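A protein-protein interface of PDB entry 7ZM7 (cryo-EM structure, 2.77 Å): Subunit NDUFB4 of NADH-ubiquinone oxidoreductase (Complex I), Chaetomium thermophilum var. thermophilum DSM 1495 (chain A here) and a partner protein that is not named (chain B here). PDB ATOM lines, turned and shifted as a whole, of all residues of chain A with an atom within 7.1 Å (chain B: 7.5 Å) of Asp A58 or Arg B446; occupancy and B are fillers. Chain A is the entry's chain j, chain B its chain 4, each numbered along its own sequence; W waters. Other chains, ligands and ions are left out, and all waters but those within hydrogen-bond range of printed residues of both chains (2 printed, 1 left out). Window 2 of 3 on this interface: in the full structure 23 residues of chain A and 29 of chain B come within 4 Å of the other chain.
NH2 of Arg B446 is in salt-bridge range of OD1 of Asp A58, 2.7 Å away.
The backbone carbonyl oxygen (O) of Leu B312 sits at hydrogen-bond distance from the guanidinium group (NH1) of Arg B446 (2.8 Å).
O of Leu A53 lies within hydrogen-bond range of OG1 of Thr A57 (2.8 Å).
The backbone carbonyl oxygen of Asp A58 is in hydrogen-bond range of the guanidinium group of Arg A75 (2.6 Å).
Among the printed residues, merely in contact across the chains: Asp A58 with Leu B447, Ala A54 with Leu B447, Ala A54 with Ile B449, Thr A57 with Ile B449, Thr A57 with Leu B447, Ala A54 with Tyr B316, Tyr A55 with Tyr B316 and Leu A53 with Ile B449.
Of the printed residues of chain B, Ala A54 touches Tyr B316, Leu B447 and Ile B449.
Of the printed residues of chain B, Thr A57 touches Leu B447 and Ile B449.
Asp A58 touches two residues of chain B.
Of the printed residues of chain A, Tyr B316 touches Ala A54 (3.7 Å) and Tyr A55 (3.7 Å).
Of chain A, only Asp A58 comes within 4 Å of Arg B446.
Of the printed residues of chain A, Leu B447 touches Ala A54, Thr A57 and Asp A58.
Printed residues of chain A within 4 Å of Ile B449: Leu A53 (3.9 Å), Ala A54 (3.6 Å) and Thr A57 (3.7 Å).
The nearest residue of chain B that does not touch Asp A58 is Tyr B316 (4.3 Å).
The nearest residue of chain A that does not touch Arg B446 is Gly A59 (4.7 Å).
Printed residues of chain B that touch a printed residue of chain A: Tyr B316, Arg B446, Leu B447 and Ile B449.
Hydrophobic or aromatic side chains of chain B within 4 Å of the printed part of chain A: Tyr B316, Leu B447 and Ile B449.
Of the 11 printed residues of chain A, 5 touch a printed residue of chain B.
Water W1 bridges the backbone NH (N) of Ile B449 (2.8 Å) and the side-chain hydroxyl (OG1) of Thr A57 (3.0 Å).
Water W2 lies within hydrogen-bond range of O of Asn B313 (3.2 Å) and OD2 of Asp A58 (3.4 Å).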
ATOM      1  N   TYR A  52     -13.399 -32.608  -0.112  1.00  0.00           N
ATOM      2  CA  TYR A  52     -13.666 -33.503   1.006  1.00  0.00           C
ATOM      3  C   TYR A  52     -12.415 -34.251   1.438  1.00  0.00           C
ATOM      4  O   TYR A  52     -12.151 -34.395   2.633  1.00  0.00           O
ATOM      5  CB  TYR A  52     -14.766 -34.487   0.633  1.00  0.00           C
ATOM      6  CG  TYR A  52     -15.188 -35.331   1.796  1.00  0.00           C
ATOM      7  CD1 TYR A  52     -15.640 -34.747   2.964  1.00  0.00           C
ATOM      8  CD2 TYR A  52     -15.130 -36.706   1.738  1.00  0.00           C
ATOM      9  CE1 TYR A  52     -16.023 -35.499   4.029  1.00  0.00           C
ATOM     10  CE2 TYR A  52     -15.513 -37.468   2.805  1.00  0.00           C
ATOM     11  CZ  TYR A  52     -15.959 -36.858   3.948  1.00  0.00           C
ATOM     12  OH  TYR A  52     -16.346 -37.619   5.026  1.00  0.00           O
ATOM     13  N   LEU A  53     -11.640 -34.750   0.482  1.00  0.00           N
ATOM     14  CA  LEU A  53     -10.384 -35.397   0.830  1.00  0.00           C
ATOM     15  C   LEU A  53      -9.414 -34.405   1.450  1.00  0.00           C
ATOM     16  O   LEU A  53      -8.679 -34.741   2.383  1.00  0.00           O
ATOM     17  CB  LEU A  53      -9.785 -36.064  -0.403  1.00  0.00           C
ATOM     18  CG  LEU A  53     -10.289 -37.455  -0.777  1.00  0.00           C
ATOM     19  CD1 LEU A  53      -9.930 -38.439   0.322  1.00  0.00           C
ATOM     20  CD2 LEU A  53     -11.780 -37.499  -1.045  1.00  0.00           C
ATOM     21  N   ALA A  54      -9.407 -33.170   0.950  1.00  0.00           N
ATOM     22  CA  ALA A  54      -8.561 -32.133   1.523  1.00  0.00           C
ATOM     23  C   ALA A  54      -8.980 -31.785   2.938  1.00  0.00           C
ATOM     24  O   ALA A  54      -8.149 -31.359   3.741  1.00  0.00           O
ATOM     25  CB  ALA A  54      -8.598 -30.884   0.644  1.00  0.00           C
ATOM     26  N   TYR A  55     -10.262 -31.919   3.252  1.00  0.00           N
ATOM     27  CA  TYR A  55     -10.724 -31.623   4.601  1.00  0.00           C
ATOM     28  C   TYR A  55     -10.361 -32.734   5.571  1.00  0.00           C
ATOM     29  O   TYR A  55      -9.950 -32.470   6.707  1.00  0.00           O
ATOM     30  CB  TYR A  55     -12.228 -31.417   4.605  1.00  0.00           C
ATOM     31  CG  TYR A  55     -12.744 -31.115   5.979  1.00  0.00           C
ATOM     32  CD1 TYR A  55     -12.615 -29.853   6.511  1.00  0.00           C
ATOM     33  CD2 TYR A  55     -13.321 -32.103   6.756  1.00  0.00           C
ATOM     34  CE1 TYR A  55     -13.057 -29.578   7.757  1.00  0.00           C
ATOM     35  CE2 TYR A  55     -13.761 -31.837   8.005  1.00  0.00           C
ATOM     36  CZ  TYR A  55     -13.633 -30.570   8.507  1.00  0.00           C
ATOM     37  OH  TYR A  55     -14.088 -30.292   9.773  1.00  0.00           O
ATOM     38  N   LYS A  56     -10.572 -33.981   5.147  1.00  0.00           N
ATOM     39  CA  LYS A  56     -10.419 -35.128   6.067  1.00  0.00           C
ATOM     40  C   LYS A  56      -8.955 -35.504   6.319  1.00  0.00           C
ATOM     41  O   LYS A  56      -8.704 -36.204   7.313  1.00  0.00           O
ATOM     42  CB  LYS A  56     -11.253 -36.288   5.528  1.00  0.00           C
ATOM     43  CG  LYS A  56     -12.756 -36.052   5.520  1.00  0.00           C
ATOM     44  CD  LYS A  56     -13.352 -35.938   6.906  1.00  0.00           C
ATOM     45  CE  LYS A  56     -13.223 -37.212   7.714  1.00  0.00           C
ATOM     46  NZ  LYS A  56     -13.814 -37.067   9.065  1.00  0.00           N
ATOM     47  N   THR A  57      -8.037 -35.096   5.450  1.00  0.00           N
ATOM     48  CA  THR A  57      -6.623 -35.502   5.628  1.00  0.00           C
ATOM     49  C   THR A  57      -5.799 -34.333   6.159  1.00  0.00           C
ATOM     50  O   THR A  57      -4.571 -34.475   6.205  1.00  0.00           O
ATOM     51  CB  THR A  57      -6.010 -36.010   4.320  1.00  0.00           C
ATOM     52  OG1 THR A  57      -6.095 -34.952   3.366  1.00  0.00           O
ATOM     53  CG2 THR A  57      -6.698 -37.244   3.781  1.00  0.00           C
ATOM     54  N   ASP A  58      -6.429 -33.206   6.490  1.00  0.00           N
ATOM     55  CA  ASP A  58      -5.650 -32.018   6.911  1.00  0.00           C
ATOM     56  C   ASP A  58      -4.893 -32.370   8.189  1.00  0.00           C
ATOM     57  O   ASP A  58      -5.522 -32.908   9.096  1.00  0.00           O
ATOM     58  CB  ASP A  58      -6.570 -30.820   7.121  1.00  0.00           C
ATOM     59  CG  ASP A  58      -5.997 -29.510   6.622  1.00  0.00           C
ATOM     60  OD1 ASP A  58      -4.853 -29.519   6.134  1.00  0.00           O
ATOM     61  OD2 ASP A  58      -6.706 -28.496   6.719  1.00  0.00           O
ATOM     62  N   GLY A  59      -3.606 -32.044   8.265  1.00  0.00           N
ATOM     63  CA  GLY A  59      -2.774 -32.373   9.438  1.00  0.00           C
ATOM     64  C   GLY A  59      -2.850 -33.826   9.862  1.00  0.00           C
ATOM     65  O   GLY A  59      -2.508 -34.106  11.022  1.00  0.00           O
ATOM     66  N   LEU A  60      -3.220 -34.727   8.954  1.00  0.00           N
ATOM     67  CA  LEU A  60      -3.394 -36.145   9.359  1.00  0.00           C
ATOM     68  C   LEU A  60      -2.001 -36.768   9.476  1.00  0.00           C
ATOM     69  O   LEU A  60      -1.799 -37.581  10.389  1.00  0.00           O
ATOM     70  CB  LEU A  60      -4.254 -36.884   8.332  1.00  0.00           C
ATOM     71  CG  LEU A  60      -4.724 -38.278   8.740  1.00  0.00           C
ATOM     72  CD1 LEU A  60      -5.254 -38.279  10.166  1.00  0.00           C
ATOM     73  CD2 LEU A  60      -5.784 -38.790   7.779  1.00  0.00           C
ATOM     74  N   TRP A  61      -1.079 -36.399   8.579  1.00  0.00           N
ATOM     75  CA  TRP A  61       0.260 -37.050   8.561  1.00  0.00           C
ATOM     76  C   TRP A  61       1.411 -36.041   8.542  1.00  0.00           C
ATOM     77  O   TRP A  61       1.258 -34.994   7.886  1.00  0.00           O
ATOM     78  CB  TRP A  61       0.368 -37.962   7.334  1.00  0.00           C
ATOM     79  CG  TRP A  61      -0.665 -39.041   7.244  1.00  0.00           C
ATOM     80  CD1 TRP A  61      -0.821 -40.107   8.081  1.00  0.00           C
ATOM     81  CD2 TRP A  61      -1.672 -39.176   6.229  1.00  0.00           C
ATOM     82  NE1 TRP A  61      -1.866 -40.888   7.665  1.00  0.00           N
ATOM     83  CE2 TRP A  61      -2.406 -40.343   6.531  1.00  0.00           C
ATOM     84  CE3 TRP A  61      -2.029 -38.425   5.105  1.00  0.00           C
ATOM     85  CZ2 TRP A  61      -3.473 -40.772   5.744  1.00  0.00           C
ATOM     86  CZ3 TRP A  61      -3.083 -38.849   4.328  1.00  0.00           C
ATOM     87  CH2 TRP A  61      -3.795 -40.006   4.646  1.00  0.00           C
ATOM     88  N   ARG A  75      -2.673 -37.522  14.202  1.00  0.00           N
ATOM     89  CA  ARG A  75      -3.992 -37.358  14.790  1.00  0.00           C
ATOM     90  C   ARG A  75      -4.740 -38.681  14.839  1.00  0.00           C
ATOM     91  O   ARG A  75      -5.539 -38.930  15.740  1.00  0.00           O
ATOM     92  CB  ARG A  75      -4.795 -36.324  14.002  1.00  0.00           C
ATOM     93  CG  ARG A  75      -6.218 -36.143  14.484  1.00  0.00           C
ATOM     94  CD  ARG A  75      -6.916 -35.008  13.762  1.00  0.00           C
ATOM     95  NE  ARG A  75      -7.169 -35.274  12.350  1.00  0.00           N
ATOM     96  CZ  ARG A  75      -6.483 -34.728  11.355  1.00  0.00           C
ATOM     97  NH1 ARG A  75      -6.791 -34.999  10.098  1.00  0.00           N
ATOM     98  NH2 ARG A  75      -5.494 -33.898  11.619  1.00  0.00           N
ATOM     99  OXT ARG A  75      -4.556 -39.538  13.978  1.00  0.00           O
ATOM    100  N   ALA B 310      -7.697 -17.557   9.711  1.00  0.00           N
ATOM    101  CA  ALA B 310      -8.590 -17.787   8.556  1.00  0.00           C
ATOM    102  C   ALA B 310      -7.827 -18.513   7.451  1.00  0.00           C
ATOM    103  O   ALA B 310      -8.305 -19.553   7.005  1.00  0.00           O
ATOM    104  CB  ALA B 310      -9.121 -16.467   8.089  1.00  0.00           C
ATOM    105  N   SER B 311      -6.661 -18.001   7.071  1.00  0.00           N
ATOM    106  CA  SER B 311      -5.827 -18.630   6.054  1.00  0.00           C
ATOM    107  C   SER B 311      -5.563 -20.091   6.389  1.00  0.00           C
ATOM    108  O   SER B 311      -5.656 -20.959   5.519  1.00  0.00           O
ATOM    109  CB  SER B 311      -4.520 -17.849   5.927  1.00  0.00           C
ATOM    110  OG  SER B 311      -3.644 -18.417   4.980  1.00  0.00           O
ATOM    111  N   LEU B 312      -5.279 -20.384   7.656  1.00  0.00           N
ATOM    112  CA  LEU B 312      -4.990 -21.751   8.078  1.00  0.00           C
ATOM    113  C   LEU B 312      -6.208 -22.661   7.960  1.00  0.00           C
ATOM    114  O   LEU B 312      -6.114 -23.766   7.424  1.00  0.00           O
ATOM    115  CB  LEU B 312      -4.479 -21.738   9.517  1.00  0.00           C
ATOM    116  CG  LEU B 312      -3.824 -22.990  10.082  1.00  0.00           C
ATOM    117  CD1 LEU B 312      -2.631 -23.395   9.263  1.00  0.00           C
ATOM    118  CD2 LEU B 312      -3.411 -22.732  11.491  1.00  0.00           C
ATOM    119  N   ASN B 313      -7.356 -22.220   8.463  1.00  0.00           N
ATOM    120  CA  ASN B 313      -8.539 -23.067   8.535  1.00  0.00           C
ATOM    121  C   ASN B 313      -9.278 -23.191   7.216  1.00  0.00           C
ATOM    122  O   ASN B 313     -10.100 -24.095   7.070  1.00  0.00           O
ATOM    123  CB  ASN B 313      -9.508 -22.535   9.580  1.00  0.00           C
ATOM    124  CG  ASN B 313      -9.357 -23.218  10.903  1.00  0.00           C
ATOM    125  OD1 ASN B 313      -8.410 -23.956  11.125  1.00  0.00           O
ATOM    126  ND2 ASN B 313     -10.296 -22.981  11.800  1.00  0.00           N
ATOM    127  N   LEU B 314      -9.014 -22.309   6.263  1.00  0.00           N
ATOM    128  CA  LEU B 314      -9.666 -22.341   4.970  1.00  0.00           C
ATOM    129  C   LEU B 314      -8.759 -22.833   3.855  1.00  0.00           C
ATOM    130  O   LEU B 314      -9.194 -22.872   2.703  1.00  0.00           O
ATOM    131  CB  LEU B 314     -10.197 -20.953   4.628  1.00  0.00           C
ATOM    132  CG  LEU B 314     -11.347 -20.383   5.456  1.00  0.00           C
ATOM    133  CD1 LEU B 314     -11.558 -18.944   5.113  1.00  0.00           C
ATOM    134  CD2 LEU B 314     -12.622 -21.161   5.263  1.00  0.00           C
ATOM    135  N   THR B 315      -7.520 -23.222   4.167  1.00  0.00           N
ATOM    136  CA  THR B 315      -6.565 -23.581   3.123  1.00  0.00           C
ATOM    137  C   THR B 315      -7.075 -24.732   2.270  1.00  0.00           C
ATOM    138  O   THR B 315      -6.824 -24.782   1.064  1.00  0.00           O
ATOM    139  CB  THR B 315      -5.209 -23.935   3.742  1.00  0.00           C
ATOM    140  OG1 THR B 315      -4.543 -22.739   4.150  1.00  0.00           O
ATOM    141  CG2 THR B 315      -4.329 -24.669   2.757  1.00  0.00           C
ATOM    142  N   TYR B 316      -7.804 -25.661   2.875  1.00  0.00           N
ATOM    143  CA  TYR B 316      -8.307 -26.794   2.119  1.00  0.00           C
ATOM    144  C   TYR B 316      -9.252 -26.350   1.011  1.00  0.00           C
ATOM    145  O   TYR B 316      -9.347 -27.021  -0.018  1.00  0.00           O
ATOM    146  CB  TYR B 316      -8.962 -27.790   3.079  1.00  0.00           C
ATOM    147  CG  TYR B 316     -10.325 -27.401   3.572  1.00  0.00           C
ATOM    148  CD1 TYR B 316     -10.476 -26.521   4.626  1.00  0.00           C
ATOM    149  CD2 TYR B 316     -11.455 -27.948   3.016  1.00  0.00           C
ATOM    150  CE1 TYR B 316     -11.711 -26.172   5.077  1.00  0.00           C
ATOM    151  CE2 TYR B 316     -12.683 -27.612   3.462  1.00  0.00           C
ATOM    152  CZ  TYR B 316     -12.811 -26.721   4.497  1.00  0.00           C
ATOM    153  OH  TYR B 316     -14.054 -26.372   4.955  1.00  0.00           O
ATOM    154  N   ILE B 317      -9.947 -25.227   1.189  1.00  0.00           N
ATOM    155  CA  ILE B 317     -10.788 -24.705   0.114  1.00  0.00           C
ATOM    156  C   ILE B 317      -9.937 -24.109  -0.996  1.00  0.00           C
ATOM    157  O   ILE B 317     -10.222 -24.290  -2.180  1.00  0.00           O
ATOM    158  CB  ILE B 317     -11.805 -23.689   0.654  1.00  0.00           C
ATOM    159  CG1 ILE B 317     -12.769 -24.366   1.600  1.00  0.00           C
ATOM    160  CG2 ILE B 317     -12.594 -23.085  -0.477  1.00  0.00           C
ATOM    161  CD1 ILE B 317     -13.434 -25.525   0.968  1.00  0.00           C
ATOM    162  N   TYR B 319      -6.858 -25.014  -1.728  1.00  0.00           N
ATOM    163  CA  TYR B 319      -6.136 -26.089  -2.394  1.00  0.00           C
ATOM    164  C   TYR B 319      -7.029 -26.861  -3.348  1.00  0.00           C
ATOM    165  O   TYR B 319      -6.581 -27.273  -4.420  1.00  0.00           O
ATOM    166  CB  TYR B 319      -5.517 -27.016  -1.356  1.00  0.00           C
ATOM    167  CG  TYR B 319      -4.159 -26.548  -0.908  1.00  0.00           C
ATOM    168  CD1 TYR B 319      -3.801 -25.209  -0.997  1.00  0.00           C
ATOM    169  CD2 TYR B 319      -3.228 -27.435  -0.407  1.00  0.00           C
ATOM    170  CE1 TYR B 319      -2.575 -24.776  -0.591  1.00  0.00           C
ATOM    171  CE2 TYR B 319      -1.992 -26.998   0.007  1.00  0.00           C
ATOM    172  CZ  TYR B 319      -1.673 -25.668  -0.095  1.00  0.00           C
ATOM    173  OH  TYR B 319      -0.442 -25.226   0.305  1.00  0.00           O
ATOM    174  N   MET B 356      -1.033 -21.912  -4.555  1.00  0.00           N
ATOM    175  CA  MET B 356      -0.999 -23.018  -3.578  1.00  0.00           C
ATOM    176  C   MET B 356       0.277 -22.900  -2.749  1.00  0.00           C
ATOM    177  O   MET B 356       0.234 -23.262  -1.574  1.00  0.00           O
ATOM    178  CB  MET B 356      -1.115 -24.354  -4.318  1.00  0.00           C
ATOM    179  CG  MET B 356      -2.523 -24.586  -4.832  1.00  0.00           C
ATOM    180  SD  MET B 356      -2.719 -26.031  -5.898  1.00  0.00           S
ATOM    181  CE  MET B 356      -3.131 -27.289  -4.694  1.00  0.00           C
ATOM    182  N   PHE B 359      -0.022 -20.400   0.217  1.00  0.00           N
ATOM    183  CA  PHE B 359      -0.944 -20.812   1.260  1.00  0.00           C
ATOM    184  C   PHE B 359      -0.458 -22.057   1.983  1.00  0.00           C
ATOM    185  O   PHE B 359      -1.236 -22.728   2.657  1.00  0.00           O
ATOM    186  CB  PHE B 359      -2.345 -21.005   0.681  1.00  0.00           C
ATOM    187  CG  PHE B 359      -3.155 -19.746   0.643  1.00  0.00           C
ATOM    188  CD1 PHE B 359      -3.815 -19.296   1.767  1.00  0.00           C
ATOM    189  CD2 PHE B 359      -3.255 -19.007  -0.518  1.00  0.00           C
ATOM    190  CE1 PHE B 359      -4.555 -18.143   1.728  1.00  0.00           C
ATOM    191  CE2 PHE B 359      -3.999 -17.865  -0.559  1.00  0.00           C
ATOM    192  CZ  PHE B 359      -4.648 -17.429   0.561  1.00  0.00           C
ATOM    193  N   SER B 360       0.853 -22.277   1.982  1.00  0.00           N
ATOM    194  CA  SER B 360       1.440 -23.506   2.574  1.00  0.00           C
ATOM    195  C   SER B 360       1.902 -23.308   4.020  1.00  0.00           C
ATOM    196  O   SER B 360       2.125 -24.329   4.681  1.00  0.00           O
ATOM    197  CB  SER B 360       2.580 -23.937   1.709  1.00  0.00           C
ATOM    198  OG  SER B 360       3.537 -22.903   1.562  1.00  0.00           O
ATOM    199  N   ASN B 361       2.094 -22.066   4.471  1.00  0.00           N
ATOM    200  CA  ASN B 361       2.605 -21.759   5.836  1.00  0.00           C
ATOM    201  C   ASN B 361       4.010 -22.324   5.973  1.00  0.00           C
ATOM    202  O   ASN B 361       4.416 -22.657   7.087  1.00  0.00           O
ATOM    203  CB  ASN B 361       1.648 -22.153   6.963  1.00  0.00           C
ATOM    204  CG  ASN B 361       1.500 -21.061   7.994  1.00  0.00           C
ATOM    205  OD1 ASN B 361       2.168 -20.038   7.910  1.00  0.00           O
ATOM    206  ND2 ASN B 361       0.623 -21.273   8.960  1.00  0.00           N
ATOM    207  N   THR B 362       4.726 -22.397   4.866  1.00  0.00           N
ATOM    208  CA  THR B 362       6.099 -22.947   4.880  1.00  0.00           C
ATOM    209  C   THR B 362       7.012 -21.890   4.267  1.00  0.00           C
ATOM    210  O   THR B 362       6.556 -21.178   3.378  1.00  0.00           O
ATOM    211  CB  THR B 362       6.144 -24.297   4.153  1.00  0.00           C
ATOM    212  OG1 THR B 362       5.150 -25.157   4.711  1.00  0.00           O
ATOM    213  CG2 THR B 362       7.488 -24.984   4.241  1.00  0.00           C
ATOM    214  N   LEU B 440       5.642 -26.698  -5.093  1.00  0.00           N
ATOM    215  CA  LEU B 440       4.985 -27.983  -4.911  1.00  0.00           C
ATOM    216  C   LEU B 440       5.353 -28.602  -3.580  1.00  0.00           C
ATOM    217  O   LEU B 440       4.507 -29.215  -2.923  1.00  0.00           O
ATOM    218  CB  LEU B 440       5.338 -28.918  -6.060  1.00  0.00           C
ATOM    219  CG  LEU B 440       4.765 -28.549  -7.432  1.00  0.00           C
ATOM    220  CD1 LEU B 440       5.169 -29.573  -8.450  1.00  0.00           C
ATOM    221  CD2 LEU B 440       3.255 -28.392  -7.429  1.00  0.00           C
ATOM    222  N   TYR B 441       6.604 -28.444  -3.153  1.00  0.00           N
ATOM    223  CA  TYR B 441       7.017 -29.018  -1.880  1.00  0.00           C
ATOM    224  C   TYR B 441       6.170 -28.479  -0.736  1.00  0.00           C
ATOM    225  O   TYR B 441       5.656 -29.247   0.080  1.00  0.00           O
ATOM    226  CB  TYR B 441       8.497 -28.748  -1.620  1.00  0.00           C
ATOM    227  CG  TYR B 441       8.879 -29.121  -0.216  1.00  0.00           C
ATOM    228  CD1 TYR B 441       9.180 -30.426   0.113  1.00  0.00           C
ATOM    229  CD2 TYR B 441       8.893 -28.187   0.793  1.00  0.00           C
ATOM    230  CE1 TYR B 441       9.496 -30.774   1.380  1.00  0.00           C
ATOM    231  CE2 TYR B 441       9.193 -28.543   2.065  1.00  0.00           C
ATOM    232  CZ  TYR B 441       9.489 -29.840   2.353  1.00  0.00           C
ATOM    233  OH  TYR B 441       9.818 -30.196   3.633  1.00  0.00           O
ATOM    234  N   GLY B 442       6.028 -27.158  -0.645  1.00  0.00           N
ATOM    235  CA  GLY B 442       5.228 -26.591   0.426  1.00  0.00           C
ATOM    236  C   GLY B 442       3.762 -26.966   0.323  1.00  0.00           C
ATOM    237  O   GLY B 442       3.117 -27.265   1.327  1.00  0.00           O
ATOM    238  N   THR B 443       3.221 -26.988  -0.890  1.00  0.00           N
ATOM    239  CA  THR B 443       1.822 -27.459  -1.053  1.00  0.00           C
ATOM    240  C   THR B 443       1.693 -28.858  -0.432  1.00  0.00           C
ATOM    241  O   THR B 443       0.721 -29.082   0.304  1.00  0.00           O
ATOM    242  CB  THR B 443       1.377 -27.343  -2.519  1.00  0.00           C
ATOM    243  OG1 THR B 443       1.565 -25.992  -2.938  1.00  0.00           O
ATOM    244  CG2 THR B 443      -0.054 -27.765  -2.755  1.00  0.00           C
ATOM    245  N   LEU B 444       2.636 -29.757  -0.719  1.00  0.00           N
ATOM    246  CA  LEU B 444       2.604 -31.147  -0.184  1.00  0.00           C
ATOM    247  C   LEU B 444       2.775 -31.196   1.338  1.00  0.00           C
ATOM    248  O   LEU B 444       2.018 -31.917   1.985  1.00  0.00           O
ATOM    249  CB  LEU B 444       3.716 -31.951  -0.866  1.00  0.00           C
ATOM    250  CG  LEU B 444       3.744 -33.440  -0.526  1.00  0.00           C
ATOM    251  CD1 LEU B 444       3.142 -34.262  -1.653  1.00  0.00           C
ATOM    252  CD2 LEU B 444       5.160 -33.901  -0.224  1.00  0.00           C
ATOM    253  N   GLU B 445       3.725 -30.449   1.894  1.00  0.00           N
ATOM    254  CA  GLU B 445       3.994 -30.539   3.355  1.00  0.00           C
ATOM    255  C   GLU B 445       2.763 -30.048   4.123  1.00  0.00           C
ATOM    256  O   GLU B 445       2.474 -30.612   5.191  1.00  0.00           O
ATOM    257  CB  GLU B 445       5.262 -29.764   3.716  1.00  0.00           C
ATOM    258  CG  GLU B 445       5.576 -29.780   5.200  1.00  0.00           C
ATOM    259  CD  GLU B 445       6.922 -29.199   5.592  1.00  0.00           C
ATOM    260  OE1 GLU B 445       7.445 -28.359   4.836  1.00  0.00           O
ATOM    261  OE2 GLU B 445       7.448 -29.595   6.648  1.00  0.00           O
ATOM    262  N   ARG B 446       2.043 -29.072   3.567  1.00  0.00           N
ATOM    263  CA  ARG B 446       0.846 -28.497   4.239  1.00  0.00           C
ATOM    264  C   ARG B 446      -0.345 -29.440   4.121  1.00  0.00           C
ATOM    265  O   ARG B 446      -0.847 -29.875   5.169  1.00  0.00           O
ATOM    266  CB  ARG B 446       0.471 -27.165   3.585  1.00  0.00           C
ATOM    267  CG  ARG B 446      -0.827 -26.556   4.090  1.00  0.00           C
ATOM    268  CD  ARG B 446      -0.779 -26.193   5.562  1.00  0.00           C
ATOM    269  NE  ARG B 446      -2.045 -25.622   5.993  1.00  0.00           N
ATOM    270  CZ  ARG B 446      -3.067 -26.328   6.461  1.00  0.00           C
ATOM    271  NH1 ARG B 446      -4.182 -25.718   6.819  1.00  0.00           N
ATOM    272  NH2 ARG B 446      -2.969 -27.640   6.574  1.00  0.00           N
ATOM    273  N   LEU B 447      -0.772 -29.812   2.954  1.00  0.00           N
ATOM    274  CA  LEU B 447      -1.893 -30.764   2.699  1.00  0.00           C
ATOM    275  C   LEU B 447      -1.392 -31.784   1.650  1.00  0.00           C
ATOM    276  O   LEU B 447      -1.527 -31.474   0.450  1.00  0.00           O
ATOM    277  CB  LEU B 447      -3.077 -29.953   2.174  1.00  0.00           C
ATOM    278  CG  LEU B 447      -4.417 -30.676   2.083  1.00  0.00           C
ATOM    279  CD1 LEU B 447      -4.629 -31.585   3.282  1.00  0.00           C
ATOM    280  CD2 LEU B 447      -5.540 -29.660   1.975  1.00  0.00           C
ATOM    281  N   PRO B 448      -0.820 -32.931   1.966  1.00  0.00           N
ATOM    282  CA  PRO B 448      -0.197 -33.857   1.006  1.00  0.00           C
ATOM    283  C   PRO B 448      -1.011 -34.338  -0.198  1.00  0.00           C
ATOM    284  O   PRO B 448      -0.396 -34.731  -1.165  1.00  0.00           O
ATOM    285  CB  PRO B 448       0.156 -35.088   1.856  1.00  0.00           C
ATOM    286  CG  PRO B 448       0.301 -34.553   3.258  1.00  0.00           C
ATOM    287  CD  PRO B 448      -0.669 -33.395   3.346  1.00  0.00           C
ATOM    288  N   ILE B 449      -2.339 -34.275  -0.144  1.00  0.00           N
ATOM    289  CA  ILE B 449      -3.142 -34.871  -1.251  1.00  0.00           C
ATOM    290  C   ILE B 449      -3.240 -33.879  -2.412  1.00  0.00           C
ATOM    291  O   ILE B 449      -3.176 -34.330  -3.567  1.00  0.00           O
ATOM    292  CB  ILE B 449      -4.521 -35.370  -0.768  1.00  0.00           C
ATOM    293  CG1 ILE B 449      -5.378 -34.258  -0.157  1.00  0.00           C
ATOM    294  CG2 ILE B 449      -4.372 -36.556   0.173  1.00  0.00           C
ATOM    295  CD1 ILE B 449      -6.486 -33.778  -1.063  1.00  0.00           C
HETATM  296  O   HOH W   1      -3.190 -34.630   2.536  1.00  0.00           O
HETATM  297  O   HOH W   2      -8.874 -26.674   8.600  1.00  0.00           O
